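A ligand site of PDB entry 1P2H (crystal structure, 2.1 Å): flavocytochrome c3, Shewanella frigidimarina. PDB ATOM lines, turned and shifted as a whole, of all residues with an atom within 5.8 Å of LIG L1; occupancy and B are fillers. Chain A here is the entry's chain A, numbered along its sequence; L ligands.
An oxygen (O3) of LIG L1 is in hydrogen-bond range of a nitrogen (N8) of LG2 L2.
An oxygen (O2) of LIG L1 is in hydrogen-bond range of the backbone NH (N) of Glu 378. An oxygen (O8) of LG2 L2 sits at hydrogen-bond distance from the backbone NH (N) of Gly 170 (3.1 Å). NH2 of Arg 402 is in salt-bridge range of O2 of LIG L1 (3.3 Å). The backbone NH of Ala 169 sits at hydrogen-bond distance from an oxygen (O8) of LG2 L2 (3.1 Å). The backbone NH of Gly 547 sits close to an oxygen (O7) of LG2 L2 (3.4 Å). An oxygen (O7) of LG2 L2 lies within hydrogen-bond range of the backbone NH (N) of Ala 549, at 2.9 Å. N of Gly 171 is in hydrogen-bond range of O8 of LG2 L2, 3.0 Å away. O4 of LIG L1 is in hydrogen-bond range of NH1 of Arg 544 (2.6 Å). The side-chain hydroxyl (OG1) of Thr 377 lies within hydrogen-bond range of an oxygen (O1) of LIG L1, 2.5 Å away. N of Gly 170 lies within hydrogen-bond range of O1 of LIG L1 (2.7 Å). A nitrogen (N7) of LG2 L2 lies within hydrogen-bond range of the backbone carbonyl oxygen (O) of Gly 171 (2.8 Å). NE2 of His 504 is in hydrogen-bond range of O5 of LIG L1 (2.7 Å). A ring nitrogen (NE2) of His 365 lies within hydrogen-bond range of an oxygen (O2) of LIG L1, at 3.0 Å. The backbone NH (N) of Gly 547 is in hydrogen-bond range of an oxygen (O4) of LIG L1, 2.7 Å away.
A ring nitrogen (NE2) of His 365 lies within hydrogen-bond range of the side-chain sulfur of Met 375, at 3.6 Å. The backbone carbonyl oxygen of Gln 363 sits at hydrogen-bond distance from the backbone NH of His 504, 2.9 Å away. The side-chain amide nitrogen of Gln 363 is in hydrogen-bond range of the backbone carbonyl oxygen of Arg 544 (2.9 Å). N of Ala 379 is in hydrogen-bond range of OG1 of Thr 377 (3.0 Å). The guanidinium group (NE) of Arg 402 lies within salt-bridge range of the side-chain carboxylate (OE1) of Glu 378 (2.7 Å). NH1 of Arg 402 sits at hydrogen-bond distance from OE1 of Gln 363 (2.9 Å). SD of Met 236 lies within hydrogen-bond range of N of Ala 379 (3.5 Å). OG1 of Thr 377 sits at hydrogen-bond distance from N of Gly 170 (3.1 Å).
Residues that only touch LIG L1: Met 375, Gly 546, Met 236, Ala 169 and Leu 545. Hydrophobic or aromatic side chains within 4 Å of LIG L1: Ala 169, Met 236, His 365, Met 375 and His 504. Within 4 Å of LIG L1: Ala 169, Gly 170, Met 236, His 365, Met 375, Thr 377, Glu 378, Arg 402, His 504, Arg 544, Leu 545, Gly 546 and Gly 547. The nearest printed residue that does not touch LIG L1 is Asn 548 (4.4 Å).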
ATOM      1  N   ALA A 168      -5.800  31.602  -6.948  1.00  0.00           N
ATOM      2  CA  ALA A 168      -7.020  31.693  -6.202  1.00  0.00           C
ATOM      3  C   ALA A 168      -8.082  32.465  -6.966  1.00  0.00           C
ATOM      4  O   ALA A 168      -7.789  33.416  -7.723  1.00  0.00           O
ATOM      5  CB  ALA A 168      -6.791  32.173  -4.764  1.00  0.00           C
ATOM      6  N   ALA A 169      -9.310  32.039  -6.749  1.00  0.00           N
ATOM      7  CA  ALA A 169     -10.442  32.558  -7.495  1.00  0.00           C
ATOM      8  C   ALA A 169     -11.508  33.189  -6.635  1.00  0.00           C
ATOM      9  O   ALA A 169     -11.598  34.413  -6.729  1.00  0.00           O
ATOM     10  CB  ALA A 169     -11.066  31.475  -8.405  1.00  0.00           C
ATOM     11  N   GLY A 170     -12.371  32.377  -6.011  1.00  0.00           N
ATOM     12  CA  GLY A 170     -13.598  32.760  -5.334  1.00  0.00           C
ATOM     13  C   GLY A 170     -13.390  33.834  -4.260  1.00  0.00           C
ATOM     14  O   GLY A 170     -14.336  34.629  -4.093  1.00  0.00           O
ATOM     15  N   GLY A 171     -12.269  33.814  -3.530  1.00  0.00           N
ATOM     16  CA  GLY A 171     -12.111  34.896  -2.554  1.00  0.00           C
ATOM     17  C   GLY A 171     -11.425  34.719  -1.220  1.00  0.00           C
ATOM     18  O   GLY A 171     -10.947  33.625  -0.869  1.00  0.00           O
ATOM     19  N   MET A 236     -19.676  31.392  -0.301  1.00  0.00           N
ATOM     20  CA  MET A 236     -18.952  30.173  -0.595  1.00  0.00           C
ATOM     21  C   MET A 236     -19.532  29.051   0.230  1.00  0.00           C
ATOM     22  O   MET A 236     -20.346  29.278   1.149  1.00  0.00           O
ATOM     23  CB  MET A 236     -17.464  30.359  -0.342  1.00  0.00           C
ATOM     24  CG  MET A 236     -16.788  31.303  -1.326  1.00  0.00           C
ATOM     25  SD  MET A 236     -16.418  30.623  -2.912  1.00  0.00           S
ATOM     26  CE  MET A 236     -14.817  29.932  -2.868  1.00  0.00           C
ATOM     27  N   GLN A 363      -8.425  18.084   1.716  1.00  0.00           N
ATOM     28  CA  GLN A 363      -9.664  18.462   1.043  1.00  0.00           C
ATOM     29  C   GLN A 363      -9.592  18.185  -0.454  1.00  0.00           C
ATOM     30  O   GLN A 363      -8.625  18.440  -1.178  1.00  0.00           O
ATOM     31  CB  GLN A 363      -9.821  20.009   1.202  1.00  0.00           C
ATOM     32  CG  GLN A 363     -11.078  20.547   0.404  1.00  0.00           C
ATOM     33  CD  GLN A 363     -11.369  21.887   1.030  1.00  0.00           C
ATOM     34  OE1 GLN A 363     -11.053  23.013   0.610  1.00  0.00           O
ATOM     35  NE2 GLN A 363     -12.124  21.837   2.144  1.00  0.00           N
ATOM     36  N   HIS A 365     -11.398  19.520  -3.835  1.00  0.00           N
ATOM     37  CA  HIS A 365     -12.350  20.525  -4.320  1.00  0.00           C
ATOM     38  C   HIS A 365     -13.419  19.756  -5.153  1.00  0.00           C
ATOM     39  O   HIS A 365     -13.077  18.916  -6.047  1.00  0.00           O
ATOM     40  CB  HIS A 365     -11.592  21.469  -5.218  1.00  0.00           C
ATOM     41  CG  HIS A 365     -12.414  22.695  -5.526  1.00  0.00           C
ATOM     42  ND1 HIS A 365     -13.475  22.715  -6.311  1.00  0.00           N
ATOM     43  CD2 HIS A 365     -12.221  23.990  -5.232  1.00  0.00           C
ATOM     44  CE1 HIS A 365     -13.952  23.909  -6.456  1.00  0.00           C
ATOM     45  NE2 HIS A 365     -13.237  24.727  -5.738  1.00  0.00           N
ATOM     46  N   MET A 375      -9.513  23.703 -11.775  1.00  0.00           N
ATOM     47  CA  MET A 375     -10.554  23.953 -10.827  1.00  0.00           C
ATOM     48  C   MET A 375     -11.539  25.013 -11.341  1.00  0.00           C
ATOM     49  O   MET A 375     -11.113  26.004 -11.969  1.00  0.00           O
ATOM     50  CB  MET A 375      -9.786  24.414  -9.576  1.00  0.00           C
ATOM     51  CG  MET A 375     -10.648  24.646  -8.378  1.00  0.00           C
ATOM     52  SD  MET A 375     -11.449  26.259  -8.505  1.00  0.00           S
ATOM     53  CE  MET A 375     -10.230  27.137  -7.478  1.00  0.00           C
ATOM     54  N   VAL A 376     -12.838  24.875 -11.061  1.00  0.00           N
ATOM     55  CA  VAL A 376     -13.898  25.818 -11.395  1.00  0.00           C
ATOM     56  C   VAL A 376     -14.402  26.434 -10.075  1.00  0.00           C
ATOM     57  O   VAL A 376     -14.740  25.628  -9.207  1.00  0.00           O
ATOM     58  CB  VAL A 376     -15.053  25.217 -12.184  1.00  0.00           C
ATOM     59  CG1 VAL A 376     -16.054  26.287 -12.607  1.00  0.00           C
ATOM     60  CG2 VAL A 376     -14.493  24.508 -13.448  1.00  0.00           C
ATOM     61  N   THR A 377     -14.212  27.723  -9.848  1.00  0.00           N
ATOM     62  CA  THR A 377     -14.458  28.272  -8.499  1.00  0.00           C
ATOM     63  C   THR A 377     -15.883  27.910  -8.076  1.00  0.00           C
ATOM     64  O   THR A 377     -16.886  27.789  -8.757  1.00  0.00           O
ATOM     65  CB  THR A 377     -14.281  29.778  -8.488  1.00  0.00           C
ATOM     66  OG1 THR A 377     -14.473  30.355  -7.181  1.00  0.00           O
ATOM     67  CG2 THR A 377     -15.321  30.469  -9.410  1.00  0.00           C
ATOM     68  N   GLU A 378     -15.985  27.570  -6.801  1.00  0.00           N
ATOM     69  CA  GLU A 378     -17.067  27.382  -5.940  1.00  0.00           C
ATOM     70  C   GLU A 378     -17.883  28.696  -5.938  1.00  0.00           C
ATOM     71  O   GLU A 378     -19.126  28.527  -5.728  1.00  0.00           O
ATOM     72  CB  GLU A 378     -16.650  27.298  -4.458  1.00  0.00           C
ATOM     73  CG  GLU A 378     -17.746  26.957  -3.451  1.00  0.00           C
ATOM     74  CD  GLU A 378     -17.265  26.000  -2.364  1.00  0.00           C
ATOM     75  OE1 GLU A 378     -16.718  24.926  -2.665  1.00  0.00           O
ATOM     76  OE2 GLU A 378     -17.412  26.307  -1.190  1.00  0.00           O
ATOM     77  N   ALA A 379     -17.267  29.855  -6.241  1.00  0.00           N
ATOM     78  CA  ALA A 379     -18.052  31.092  -6.394  1.00  0.00           C
ATOM     79  C   ALA A 379     -19.109  31.077  -7.543  1.00  0.00           C
ATOM     80  O   ALA A 379     -20.042  31.879  -7.538  1.00  0.00           O
ATOM     81  CB  ALA A 379     -17.246  32.316  -6.620  1.00  0.00           C
ATOM     82  N   ARG A 402     -17.465  20.963   1.440  1.00  0.00           N
ATOM     83  CA  ARG A 402     -16.717  20.345   0.345  1.00  0.00           C
ATOM     84  C   ARG A 402     -16.627  18.843   0.413  1.00  0.00           C
ATOM     85  O   ARG A 402     -16.607  18.082  -0.557  1.00  0.00           O
ATOM     86  CB  ARG A 402     -15.315  21.040   0.211  1.00  0.00           C
ATOM     87  CG  ARG A 402     -15.273  22.223  -0.714  1.00  0.00           C
ATOM     88  CD  ARG A 402     -14.208  23.272  -0.453  1.00  0.00           C
ATOM     89  NE  ARG A 402     -14.389  24.448  -1.341  1.00  0.00           N
ATOM     90  CZ  ARG A 402     -13.363  25.208  -1.724  1.00  0.00           C
ATOM     91  NH1 ARG A 402     -12.155  24.885  -1.277  1.00  0.00           N
ATOM     92  NH2 ARG A 402     -13.563  26.237  -2.558  1.00  0.00           N
ATOM     93  N   HIS A 504      -7.074  19.192  -3.498  1.00  0.00           N
ATOM     94  CA  HIS A 504      -6.883  20.680  -3.599  1.00  0.00           C
ATOM     95  C   HIS A 504      -6.181  21.333  -2.434  1.00  0.00           C
ATOM     96  O   HIS A 504      -5.483  22.315  -2.604  1.00  0.00           O
ATOM     97  CB  HIS A 504      -8.330  21.168  -3.751  1.00  0.00           C
ATOM     98  CG  HIS A 504      -8.642  22.635  -3.685  1.00  0.00           C
ATOM     99  ND1 HIS A 504      -8.183  23.473  -4.735  1.00  0.00           N
ATOM    100  CD2 HIS A 504      -9.189  23.420  -2.778  1.00  0.00           C
ATOM    101  CE1 HIS A 504      -8.589  24.714  -4.424  1.00  0.00           C
ATOM    102  NE2 HIS A 504      -9.159  24.722  -3.243  1.00  0.00           N
ATOM    103  N   ARG A 544     -11.885  22.447   5.337  1.00  0.00           N
ATOM    104  CA  ARG A 544     -11.710  23.922   5.278  1.00  0.00           C
ATOM    105  C   ARG A 544     -12.858  24.628   4.577  1.00  0.00           C
ATOM    106  O   ARG A 544     -13.271  24.100   3.566  1.00  0.00           O
ATOM    107  CB  ARG A 544     -10.405  24.292   4.576  1.00  0.00           C
ATOM    108  CG  ARG A 544     -10.226  25.744   4.128  1.00  0.00           C
ATOM    109  CD  ARG A 544      -8.758  26.005   3.836  1.00  0.00           C
ATOM    110  NE  ARG A 544      -8.517  25.587   2.418  1.00  0.00           N
ATOM    111  CZ  ARG A 544      -9.026  26.185   1.359  1.00  0.00           C
ATOM    112  NH1 ARG A 544      -9.901  27.213   1.404  1.00  0.00           N
ATOM    113  NH2 ARG A 544      -8.741  25.775   0.165  1.00  0.00           N
ATOM    114  N   LEU A 545     -13.157  25.859   4.897  1.00  0.00           N
ATOM    115  CA  LEU A 545     -14.224  26.587   4.198  1.00  0.00           C
ATOM    116  C   LEU A 545     -13.687  27.328   2.983  1.00  0.00           C
ATOM    117  O   LEU A 545     -12.578  27.875   3.085  1.00  0.00           O
ATOM    118  CB  LEU A 545     -14.813  27.556   5.172  1.00  0.00           C
ATOM    119  CG  LEU A 545     -15.874  27.160   6.151  1.00  0.00           C
ATOM    120  CD1 LEU A 545     -16.616  28.389   6.733  1.00  0.00           C
ATOM    121  CD2 LEU A 545     -16.884  26.213   5.498  1.00  0.00           C
ATOM    122  N   GLY A 546     -14.377  27.319   1.873  1.00  0.00           N
ATOM    123  CA  GLY A 546     -13.924  28.080   0.676  1.00  0.00           C
ATOM    124  C   GLY A 546     -13.744  29.533   1.110  1.00  0.00           C
ATOM    125  O   GLY A 546     -14.565  29.986   1.911  1.00  0.00           O
ATOM    126  N   GLY A 547     -12.598  30.161   0.708  1.00  0.00           N
ATOM    127  CA  GLY A 547     -12.426  31.539   1.192  1.00  0.00           C
ATOM    128  C   GLY A 547     -11.459  31.573   2.390  1.00  0.00           C
ATOM    129  O   GLY A 547     -10.683  32.508   2.471  1.00  0.00           O
ATOM    130  N   ASN A 548     -11.433  30.549   3.266  1.00  0.00           N
ATOM    131  CA  ASN A 548     -10.529  30.658   4.376  1.00  0.00           C
ATOM    132  C   ASN A 548      -9.036  30.498   4.161  1.00  0.00           C
ATOM    133  O   ASN A 548      -8.366  30.980   5.116  1.00  0.00           O
ATOM    134  CB  ASN A 548     -10.989  29.676   5.497  1.00  0.00           C
ATOM    135  CG  ASN A 548     -12.051  30.431   6.314  1.00  0.00           C
ATOM    136  OD1 ASN A 548     -12.320  31.614   6.052  1.00  0.00           O
ATOM    137  ND2 ASN A 548     -12.627  29.737   7.215  1.00  0.00           N
ATOM    138  N   ALA A 549      -8.493  29.904   3.103  1.00  0.00           N
ATOM    139  CA  ALA A 549      -7.014  29.691   3.107  1.00  0.00           C
ATOM    140  C   ALA A 549      -6.379  31.016   2.711  1.00  0.00           C
ATOM    141  O   ALA A 549      -5.299  31.323   3.153  1.00  0.00           O
ATOM    142  CB  ALA A 549      -6.609  28.695   2.003  1.00  0.00           C
HETATM  143  C1  LIG L   1     -12.525  28.586  -5.297  1.00  0.00           C
HETATM  144  O1  LIG L   1     -12.442  29.677  -5.819  1.00  0.00           O
HETATM  145  O2  LIG L   1     -13.361  27.730  -5.489  1.00  0.00           O
HETATM  146  C2  LIG L   1     -11.483  28.058  -4.209  1.00  0.00           C
HETATM  147  O3  LIG L   1     -10.745  27.047  -4.575  1.00  0.00           O
HETATM  148  C3  LIG L   1     -11.699  28.512  -2.923  1.00  0.00           C
HETATM  149  C4  LIG L   1     -11.097  27.973  -1.845  1.00  0.00           C
HETATM  150  O4  LIG L   1     -11.135  28.362  -0.584  1.00  0.00           O
HETATM  151  O5  LIG L   1     -10.299  26.696  -1.853  1.00  0.00           O
HETATM  152  P1  LG2 L   2       1.396  28.733  -1.656  1.00  0.00           P
HETATM  153  O1  LG2 L   2       1.066  27.384  -2.218  1.00  0.00           O
HETATM  154  O2  LG2 L   2       0.692  29.907  -2.147  1.00  0.00           O
HETATM  155  O3  LG2 L   2       2.962  29.010  -1.815  1.00  0.00           O
HETATM  156  C1  LG2 L   2       4.046  28.295  -1.212  1.00  0.00           C
HETATM  157  C2  LG2 L   2       5.303  28.593  -2.035  1.00  0.00           C
HETATM  158  O4  LG2 L   2       6.411  27.888  -1.404  1.00  0.00           O
HETATM  159  C3  LG2 L   2       5.154  27.912  -3.422  1.00  0.00           C
HETATM  160  O5  LG2 L   2       5.488  28.774  -4.482  1.00  0.00           O
HETATM  161  C4  LG2 L   2       6.104  26.699  -3.290  1.00  0.00           C
HETATM  162  O6  LG2 L   2       6.774  26.513  -4.550  1.00  0.00           O
HETATM  163  C5  LG2 L   2       7.238  27.387  -2.411  1.00  0.00           C
HETATM  164  N1  LG2 L   2       8.041  26.341  -1.794  1.00  0.00           N
HETATM  165  C6  LG2 L   2       7.654  25.044  -1.433  1.00  0.00           C
HETATM  166  N2  LG2 L   2       8.566  24.347  -0.868  1.00  0.00           N
HETATM  167  C7  LG2 L   2       9.675  25.163  -0.815  1.00  0.00           C
HETATM  168  C8  LG2 L   2      11.008  25.002  -0.462  1.00  0.00           C
HETATM  169  N3  LG2 L   2      11.511  23.946   0.175  1.00  0.00           N
HETATM  170  N4  LG2 L   2      11.853  26.017  -0.783  1.00  0.00           N
HETATM  171  C9  LG2 L   2      11.436  27.138  -1.349  1.00  0.00           C
HETATM  172  N5  LG2 L   2      10.139  27.389  -1.800  1.00  0.00           N
HETATM  173  C10 LG2 L   2       9.347  26.343  -1.440  1.00  0.00           C
HETATM  174  N6  LG2 L   2      -8.110  29.446  -1.161  1.00  0.00           N
HETATM  175  C11 LG2 L   2      -9.037  30.408  -0.810  1.00  0.00           C
HETATM  176  O7  LG2 L   2      -9.236  30.643   0.353  1.00  0.00           O
HETATM  177  N7  LG2 L   2      -9.793  31.171  -1.730  1.00  0.00           N
HETATM  178  C12 LG2 L   2      -9.634  30.913  -3.101  1.00  0.00           C
HETATM  179  O8  LG2 L   2     -10.306  31.536  -3.831  1.00  0.00           O
HETATM  180  C13 LG2 L   2      -8.756  29.757  -3.453  1.00  0.00           C
HETATM  181  N8  LG2 L   2      -8.701  29.319  -4.683  1.00  0.00           N
HETATM  182  C14 LG2 L   2      -7.732  28.366  -4.943  1.00  0.00           C
HETATM  183  C15 LG2 L   2      -7.529  28.018  -6.350  1.00  0.00           C
HETATM  184  C16 LG2 L   2      -6.707  26.950  -6.658  1.00  0.00           C
HETATM  185  C17 LG2 L   2      -6.544  26.369  -8.029  1.00  0.00           C
HETATM  186  C18 LG2 L   2      -5.833  26.407  -5.607  1.00  0.00           C
HETATM  187  C19 LG2 L   2      -4.887  25.278  -5.961  1.00  0.00           C
HETATM  188  C20 LG2 L   2      -5.929  26.816  -4.241  1.00  0.00           C
HETATM  189  C21 LG2 L   2      -6.964  27.733  -3.920  1.00  0.00           C
HETATM  190  N9  LG2 L   2      -7.214  28.058  -2.602  1.00  0.00           N
HETATM  191  C22 LG2 L   2      -8.066  29.113  -2.379  1.00  0.00           C
HETATM  192  C23 LG2 L   2      -6.245  27.709  -1.544  1.00  0.00           C
HETATM  193  C24 LG2 L   2      -5.140  28.725  -1.424  1.00  0.00           C
HETATM  194  O9  LG2 L   2      -4.779  29.441  -2.667  1.00  0.00           O
HETATM  195  C25 LG2 L   2      -3.805  27.983  -0.939  1.00  0.00           C
HETATM  196  O10 LG2 L   2      -4.270  27.393   0.319  1.00  0.00           O
HETATM  197  C26 LG2 L   2      -2.668  29.020  -0.526  1.00  0.00           C
HETATM  198  O11 LG2 L   2      -2.151  29.253  -1.857  1.00  0.00           O
HETATM  199  C27 LG2 L   2      -1.678  28.579   0.542  1.00  0.00           C
HETATM  200  O12 LG2 L   2      -0.806  29.697   0.413  1.00  0.00           O
HETATM  201  P2  LG2 L   2       0.708  29.634   1.041  1.00  0.00           P
HETATM  202  O13 LG2 L   2       1.393  30.867   1.009  1.00  0.00           O
HETATM  203  O14 LG2 L   2       0.507  28.917   2.289  1.00  0.00           O
HETATM  204  O15 LG2 L   2       1.283  28.578  -0.070  1.00  0.00           O
